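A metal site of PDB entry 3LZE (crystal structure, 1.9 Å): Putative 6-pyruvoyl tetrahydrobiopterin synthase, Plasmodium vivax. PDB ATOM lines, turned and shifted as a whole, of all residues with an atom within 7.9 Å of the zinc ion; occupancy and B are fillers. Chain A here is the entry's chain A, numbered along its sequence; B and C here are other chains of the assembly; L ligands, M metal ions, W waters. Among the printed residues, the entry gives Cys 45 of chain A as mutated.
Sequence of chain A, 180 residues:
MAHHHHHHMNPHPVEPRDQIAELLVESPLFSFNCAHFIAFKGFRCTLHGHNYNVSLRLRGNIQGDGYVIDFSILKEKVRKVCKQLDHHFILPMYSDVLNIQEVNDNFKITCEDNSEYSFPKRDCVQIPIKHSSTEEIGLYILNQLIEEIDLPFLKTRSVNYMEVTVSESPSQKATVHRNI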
ATOM      1  N   CYS A  34      24.166 -31.126 -13.183  1.00  0.00           N
ATOM      2  CA  CYS A  34      23.436 -32.254 -12.673  1.00  0.00           C
ATOM      3  C   CYS A  34      22.277 -31.830 -11.788  1.00  0.00           C
ATOM      4  O   CYS A  34      22.254 -30.702 -11.278  1.00  0.00           O
ATOM      5  CB  CYS A  34      24.371 -33.137 -11.833  1.00  0.00           C
ATOM      6  SG  CYS A  34      25.572 -34.014 -12.891  1.00  0.00           S
ATOM      7  N   ALA A  35      21.296 -32.715 -11.639  1.00  0.00           N
ATOM      8  CA  ALA A  35      20.210 -32.559 -10.689  1.00  0.00           C
ATOM      9  C   ALA A  35      20.597 -33.406  -9.486  1.00  0.00           C
ATOM     10  O   ALA A  35      21.283 -34.410  -9.652  1.00  0.00           O
ATOM     11  CB  ALA A  35      18.859 -33.051 -11.259  1.00  0.00           C
ATOM     12  N   HIS A  36      20.092 -33.050  -8.321  1.00  0.00           N
ATOM     13  CA  HIS A  36      20.292 -33.882  -7.117  1.00  0.00           C
ATOM     14  C   HIS A  36      19.308 -33.383  -6.063  1.00  0.00           C
ATOM     15  O   HIS A  36      18.559 -32.423  -6.303  1.00  0.00           O
ATOM     16  CB  HIS A  36      21.697 -33.787  -6.610  1.00  0.00           C
ATOM     17  CG  HIS A  36      21.952 -32.599  -5.741  1.00  0.00           C
ATOM     18  ND1 HIS A  36      22.497 -32.721  -4.488  1.00  0.00           N
ATOM     19  CD2 HIS A  36      21.720 -31.271  -5.915  1.00  0.00           C
ATOM     20  CE1 HIS A  36      22.608 -31.522  -3.928  1.00  0.00           C
ATOM     21  NE2 HIS A  36      22.158 -30.630  -4.787  1.00  0.00           N
ATOM     22  N   PHE A  37      19.271 -34.033  -4.930  1.00  0.00           N
ATOM     23  CA  PHE A  37      18.598 -33.462  -3.823  1.00  0.00           C
ATOM     24  C   PHE A  37      19.268 -34.045  -2.607  1.00  0.00           C
ATOM     25  O   PHE A  37      19.755 -35.147  -2.652  1.00  0.00           O
ATOM     26  CB  PHE A  37      17.054 -33.685  -3.844  1.00  0.00           C
ATOM     27  CG  PHE A  37      16.602 -35.155  -3.677  1.00  0.00           C
ATOM     28  CD1 PHE A  37      16.465 -35.719  -2.410  1.00  0.00           C
ATOM     29  CD2 PHE A  37      16.096 -35.861  -4.769  1.00  0.00           C
ATOM     30  CE1 PHE A  37      15.958 -37.034  -2.245  1.00  0.00           C
ATOM     31  CE2 PHE A  37      15.596 -37.159  -4.628  1.00  0.00           C
ATOM     32  CZ  PHE A  37      15.552 -37.760  -3.345  1.00  0.00           C
ATOM     33  N   ILE A  38      19.277 -33.270  -1.532  1.00  0.00           N
ATOM     34  CA  ILE A  38      19.894 -33.642  -0.261  1.00  0.00           C
ATOM     35  C   ILE A  38      18.866 -34.301   0.617  1.00  0.00           C
ATOM     36  O   ILE A  38      17.766 -33.784   0.752  1.00  0.00           O
ATOM     37  CB  ILE A  38      20.433 -32.393   0.481  1.00  0.00           C
ATOM     38  CG1 ILE A  38      21.554 -31.735  -0.324  1.00  0.00           C
ATOM     39  CG2 ILE A  38      20.929 -32.744   1.900  1.00  0.00           C
ATOM     40  CD1 ILE A  38      22.753 -32.648  -0.575  1.00  0.00           C
ATOM     41  N   CYS A  45      15.651 -32.031   1.083  1.00  0.00           N
ATOM     42  CA  CYS A  45      15.397 -30.827   0.272  1.00  0.00           C
ATOM     43  C   CYS A  45      14.684 -31.250  -1.004  1.00  0.00           C
ATOM     44  O   CYS A  45      14.554 -32.445  -1.317  1.00  0.00           O
ATOM     45  CB  CYS A  45      16.680 -30.076  -0.096  1.00  0.00           C
ATOM     46  SG  CYS A  45      17.431 -30.585  -1.690  1.00  0.00           S
ATOM     47  N   THR A  46      14.192 -30.247  -1.712  1.00  0.00           N
ATOM     48  CA  THR A  46      13.532 -30.469  -2.967  1.00  0.00           C
ATOM     49  C   THR A  46      14.580 -30.741  -4.080  1.00  0.00           C
ATOM     50  O   THR A  46      15.741 -30.371  -3.990  1.00  0.00           O
ATOM     51  CB  THR A  46      12.655 -29.244  -3.348  1.00  0.00           C
ATOM     52  OG1 THR A  46      13.416 -28.042  -3.161  1.00  0.00           O
ATOM     53  CG2 THR A  46      11.420 -29.141  -2.422  1.00  0.00           C
ATOM     54  N   LEU A  47      14.124 -31.408  -5.122  1.00  0.00           N
ATOM     55  CA  LEU A  47      14.874 -31.564  -6.337  1.00  0.00           C
ATOM     56  C   LEU A  47      15.244 -30.236  -6.967  1.00  0.00           C
ATOM     57  O   LEU A  47      14.419 -29.328  -7.138  1.00  0.00           O
ATOM     58  CB  LEU A  47      14.043 -32.340  -7.348  1.00  0.00           C
ATOM     59  CG  LEU A  47      14.708 -32.666  -8.683  1.00  0.00           C
ATOM     60  CD1 LEU A  47      15.823 -33.654  -8.468  1.00  0.00           C
ATOM     61  CD2 LEU A  47      13.611 -33.241  -9.634  1.00  0.00           C
ATOM     62  N   HIS A  48      16.510 -30.157  -7.356  1.00  0.00           N
ATOM     63  CA  HIS A  48      17.078 -28.958  -7.948  1.00  0.00           C
ATOM     64  C   HIS A  48      18.333 -29.397  -8.667  1.00  0.00           C
ATOM     65  O   HIS A  48      18.485 -30.585  -8.939  1.00  0.00           O
ATOM     66  CB  HIS A  48      17.363 -27.914  -6.867  1.00  0.00           C
ATOM     67  CG  HIS A  48      18.407 -28.301  -5.841  1.00  0.00           C
ATOM     68  ND1 HIS A  48      18.096 -29.008  -4.690  1.00  0.00           N
ATOM     69  CD2 HIS A  48      19.705 -27.954  -5.732  1.00  0.00           C
ATOM     70  CE1 HIS A  48      19.187 -29.147  -3.966  1.00  0.00           C
ATOM     71  NE2 HIS A  48      20.179 -28.522  -4.567  1.00  0.00           N
ATOM     72  N   GLY A  49      19.265 -28.480  -8.903  1.00  0.00           N
ATOM     73  CA  GLY A  49      20.410 -28.782  -9.727  1.00  0.00           C
ATOM     74  C   GLY A  49      21.485 -27.742  -9.609  1.00  0.00           C
ATOM     75  O   GLY A  49      21.304 -26.693  -8.982  1.00  0.00           O
ATOM     76  N   HIS A  50      22.613 -28.034 -10.230  1.00  0.00           N
ATOM     77  CA  HIS A  50      23.811 -27.204 -10.164  1.00  0.00           C
ATOM     78  C   HIS A  50      24.722 -27.435 -11.343  1.00  0.00           C
ATOM     79  O   HIS A  50      24.759 -28.546 -11.913  1.00  0.00           O
ATOM     80  CB  HIS A  50      24.650 -27.549  -8.950  1.00  0.00           C
ATOM     81  CG  HIS A  50      23.969 -27.378  -7.646  1.00  0.00           C
ATOM     82  ND1 HIS A  50      23.601 -26.139  -7.140  1.00  0.00           N
ATOM     83  CD2 HIS A  50      23.594 -28.294  -6.723  1.00  0.00           C
ATOM     84  CE1 HIS A  50      23.013 -26.310  -5.964  1.00  0.00           C
ATOM     85  NE2 HIS A  50      22.990 -27.604  -5.702  1.00  0.00           N
ATOM     86  N   TYR A  52      28.140 -27.956 -11.416  1.00  0.00           N
ATOM     87  CA  TYR A  52      29.260 -28.256 -10.554  1.00  0.00           C
ATOM     88  C   TYR A  52      30.512 -27.962 -11.325  1.00  0.00           C
ATOM     89  O   TYR A  52      30.559 -28.180 -12.546  1.00  0.00           O
ATOM     90  CB  TYR A  52      29.246 -29.722 -10.129  1.00  0.00           C
ATOM     91  CG  TYR A  52      28.139 -30.127  -9.186  1.00  0.00           C
ATOM     92  CD1 TYR A  52      28.339 -30.137  -7.817  1.00  0.00           C
ATOM     93  CD2 TYR A  52      26.901 -30.577  -9.666  1.00  0.00           C
ATOM     94  CE1 TYR A  52      27.345 -30.584  -6.955  1.00  0.00           C
ATOM     95  CE2 TYR A  52      25.912 -31.029  -8.797  1.00  0.00           C
ATOM     96  CZ  TYR A  52      26.142 -31.024  -7.442  1.00  0.00           C
ATOM     97  OH  TYR A  52      25.150 -31.466  -6.563  1.00  0.00           O
ATOM     98  N   SER A 132      24.601 -36.904  -1.827  1.00  0.00           N
ATOM     99  CA  SER A 132      25.054 -36.121  -2.948  1.00  0.00           C
ATOM    100  C   SER A 132      25.511 -34.723  -2.491  1.00  0.00           C
ATOM    101  O   SER A 132      25.174 -33.705  -3.120  1.00  0.00           O
ATOM    102  CB  SER A 132      23.946 -36.033  -4.028  1.00  0.00           C
ATOM    103  OG  SER A 132      22.762 -35.433  -3.532  1.00  0.00           O
ATOM    104  N   SER A 133      26.282 -34.682  -1.408  1.00  0.00           N
ATOM    105  CA  SER A 133      26.922 -33.460  -0.954  1.00  0.00           C
ATOM    106  C   SER A 133      28.215 -33.198  -1.692  1.00  0.00           C
ATOM    107  O   SER A 133      28.871 -34.107  -2.214  1.00  0.00           O
ATOM    108  CB  SER A 133      27.249 -33.570   0.551  1.00  0.00           C
ATOM    109  OG  SER A 133      28.240 -34.558   0.763  1.00  0.00           O
ATOM    110  N   THR A 134      28.631 -31.932  -1.683  1.00  0.00           N
ATOM    111  CA  THR A 134      29.835 -31.521  -2.369  1.00  0.00           C
ATOM    112  C   THR A 134      31.064 -32.262  -1.877  1.00  0.00           C
ATOM    113  O   THR A 134      31.927 -32.656  -2.643  1.00  0.00           O
ATOM    114  CB  THR A 134      29.973 -29.999  -2.217  1.00  0.00           C
ATOM    115  OG1 THR A 134      28.721 -29.414  -2.614  1.00  0.00           O
ATOM    116  CG2 THR A 134      31.032 -29.460  -3.093  1.00  0.00           C
ATOM    117  N   GLU A 168      29.640 -26.410  -5.921  1.00  0.00           N
ATOM    118  CA  GLU A 168      28.269 -26.604  -6.365  1.00  0.00           C
ATOM    119  C   GLU A 168      27.690 -25.301  -6.904  1.00  0.00           C
ATOM    120  O   GLU A 168      26.696 -25.307  -7.640  1.00  0.00           O
ATOM    121  CB  GLU A 168      27.438 -27.159  -5.238  1.00  0.00           C
ATOM    122  CG  GLU A 168      27.371 -26.278  -4.019  1.00  0.00           C
ATOM    123  CD  GLU A 168      26.266 -26.714  -3.116  1.00  0.00           C
ATOM    124  OE1 GLU A 168      26.437 -27.755  -2.443  1.00  0.00           O
ATOM    125  OE2 GLU A 168      25.215 -26.035  -3.093  1.00  0.00           O
ATOM    126  N   GLN A 172      30.405 -21.813  -2.859  1.00  0.00           N
ATOM    127  CA  GLN A 172      30.449 -22.933  -1.900  1.00  0.00           C
ATOM    128  C   GLN A 172      31.238 -24.062  -2.521  1.00  0.00           C
ATOM    129  O   GLN A 172      30.778 -24.670  -3.529  1.00  0.00           O
ATOM    130  CB  GLN A 172      29.060 -23.489  -1.550  1.00  0.00           C
ATOM    131  CG  GLN A 172      27.943 -22.493  -1.545  1.00  0.00           C
ATOM    132  CD  GLN A 172      26.632 -23.086  -1.015  1.00  0.00           C
ATOM    133  OE1 GLN A 172      25.871 -22.395  -0.347  1.00  0.00           O
ATOM    134  NE2 GLN A 172      26.374 -24.357  -1.312  1.00  0.00           N
ATOM    135  N   ASN B  33      18.857 -22.308  -8.463  1.00  0.00           N
ATOM    136  CA  ASN B  33      19.504 -23.569  -8.704  1.00  0.00           C
ATOM    137  C   ASN B  33      18.379 -24.581  -8.955  1.00  0.00           C
ATOM    138  O   ASN B  33      17.657 -24.957  -8.023  1.00  0.00           O
ATOM    139  CB  ASN B  33      20.392 -23.910  -7.497  1.00  0.00           C
ATOM    140  CG  ASN B  33      21.465 -22.826  -7.222  1.00  0.00           C
ATOM    141  OD1 ASN B  33      21.784 -21.968  -8.082  1.00  0.00           O
ATOM    142  ND2 ASN B  33      22.004 -22.838  -6.031  1.00  0.00           N
ATOM    143  N   ASN B  51      22.800 -23.722 -12.128  1.00  0.00           N
ATOM    144  CA  ASN B  51      22.804 -22.522 -11.327  1.00  0.00           C
ATOM    145  C   ASN B  51      22.490 -21.397 -12.285  1.00  0.00           C
ATOM    146  O   ASN B  51      23.383 -20.801 -12.903  1.00  0.00           O
ATOM    147  CB  ASN B  51      24.185 -22.276 -10.669  1.00  0.00           C
ATOM    148  CG  ASN B  51      24.588 -23.393  -9.748  1.00  0.00           C
ATOM    149  OD1 ASN B  51      23.738 -23.912  -9.017  1.00  0.00           O
ATOM    150  ND2 ASN B  51      25.883 -23.773  -9.743  1.00  0.00           N
ATOM    151  N   HIS B  87      15.647 -23.925  -6.187  1.00  0.00           N
ATOM    152  CA  HIS B  87      15.465 -25.249  -5.574  1.00  0.00           C
ATOM    153  C   HIS B  87      14.196 -26.025  -6.023  1.00  0.00           C
ATOM    154  O   HIS B  87      13.505 -26.624  -5.213  1.00  0.00           O
ATOM    155  CB  HIS B  87      15.579 -25.144  -4.044  1.00  0.00           C
ATOM    156  CG  HIS B  87      16.988 -25.260  -3.568  1.00  0.00           C
ATOM    157  ND1 HIS B  87      17.369 -26.118  -2.565  1.00  0.00           N
ATOM    158  CD2 HIS B  87      18.125 -24.677  -4.020  1.00  0.00           C
ATOM    159  CE1 HIS B  87      18.679 -26.038  -2.385  1.00  0.00           C
ATOM    160  NE2 HIS B  87      19.169 -25.161  -3.252  1.00  0.00           N
ATOM    161  N   TYR C  67      27.944 -33.610   5.494  1.00  0.00           N
ATOM    162  CA  TYR C  67      28.529 -32.263   5.516  1.00  0.00           C
ATOM    163  C   TYR C  67      29.622 -32.197   6.578  1.00  0.00           C
ATOM    164  O   TYR C  67      29.479 -32.840   7.608  1.00  0.00           O
ATOM    165  CB  TYR C  67      27.488 -31.242   5.931  1.00  0.00           C
ATOM    166  CG  TYR C  67      26.284 -31.023   5.014  1.00  0.00           C
ATOM    167  CD1 TYR C  67      26.301 -31.409   3.689  1.00  0.00           C
ATOM    168  CD2 TYR C  67      25.143 -30.378   5.494  1.00  0.00           C
ATOM    169  CE1 TYR C  67      25.195 -31.164   2.862  1.00  0.00           C
ATOM    170  CE2 TYR C  67      24.044 -30.135   4.691  1.00  0.00           C
ATOM    171  CZ  TYR C  67      24.075 -30.526   3.365  1.00  0.00           C
ATOM    172  OH  TYR C  67      23.006 -30.268   2.518  1.00  0.00           O
HETATM  173  C1  LIG L   1      25.446 -28.495   0.794  1.00  0.00           C
HETATM  174  C2  LIG L   1      26.594 -29.299   0.563  1.00  0.00           C
HETATM  175  O1  LIG L   1      26.725 -30.022  -0.452  1.00  0.00           O
HETATM  176  N1  LIG L   1      27.626 -29.280   1.519  1.00  0.00           N
HETATM  177  C3  LIG L   1      27.472 -28.489   2.711  1.00  0.00           C
HETATM  178  N2  LIG L   1      28.429 -28.448   3.640  1.00  0.00           N
HETATM  179  N3  LIG L   1      26.360 -27.742   2.897  1.00  0.00           N
HETATM  180  C4  LIG L   1      25.355 -27.737   1.969  1.00  0.00           C
HETATM  181  N4  LIG L   1      24.258 -26.973   2.186  1.00  0.00           N
HETATM  182  C5  LIG L   1      23.245 -26.950   1.308  1.00  0.00           C
HETATM  183  C6  LIG L   1      23.323 -27.720   0.149  1.00  0.00           C
HETATM  184  N5  LIG L   1      24.392 -28.476  -0.084  1.00  0.00           N
HETATM  185 ZN    ZN M   1      22.114 -28.624  -4.141  1.00  0.00          ZN
HETATM  186  O   HOH W   1      21.906 -29.190  -1.983  1.00  0.00           O
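OE1 of Glu 168 lies close to N5 of the ligand (3.2 Å). An oxygen (O1) of the ligand sits at hydrogen-bond distance from the backbone NH (N) of Thr 134 (3.0 Å). OG1 of Thr 134 is in hydrogen-bond range of O1 of the ligand (3.0 Å). The side-chain hydroxyl of Tyr 67 of chain C is in hydrogen-bond range of a nitrogen (N5) of the ligand (3.5 Å).
The zinc ion is bound by a ring nitrogen (NE2) of His 48 (2.0 Å), a ring nitrogen (NE2) of His 50 (2.1 Å), a ring nitrogen (NE2) of His 36 (2.1 Å) and water W1 (2.2 Å). The zinc ion has four donor atoms within binding distance.
A ring nitrogen (ND1) of His 48 lies close to the side-chain sulfur (SG) of Cys 45. The backbone carbonyl oxygen of Thr 46 is in hydrogen-bond range of a ring nitrogen (ND1) of His 48, 2.8 Å away. ND1 of His 50 is in hydrogen-bond range of O of Glu 168, at 3.2 Å. A ring nitrogen (ND1) of His 50 lies within hydrogen-bond range of the side-chain amide oxygen of Asn 51 of chain B (2.9 Å). The backbone carbonyl oxygen (O) of Cys 34 lies within hydrogen-bond range of the backbone NH (N) of His 50 (2.9 Å). A ring nitrogen (ND1) of His 36 lies within hydrogen-bond range of the side-chain hydroxyl (OG) of Ser 132, 2.9 Å away.
Of the 21 residues printed, 3 come within 4 Å of the zinc ion. The nearest printed residue that does not touch the zinc ion is Glu 168 (4.2 Å).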
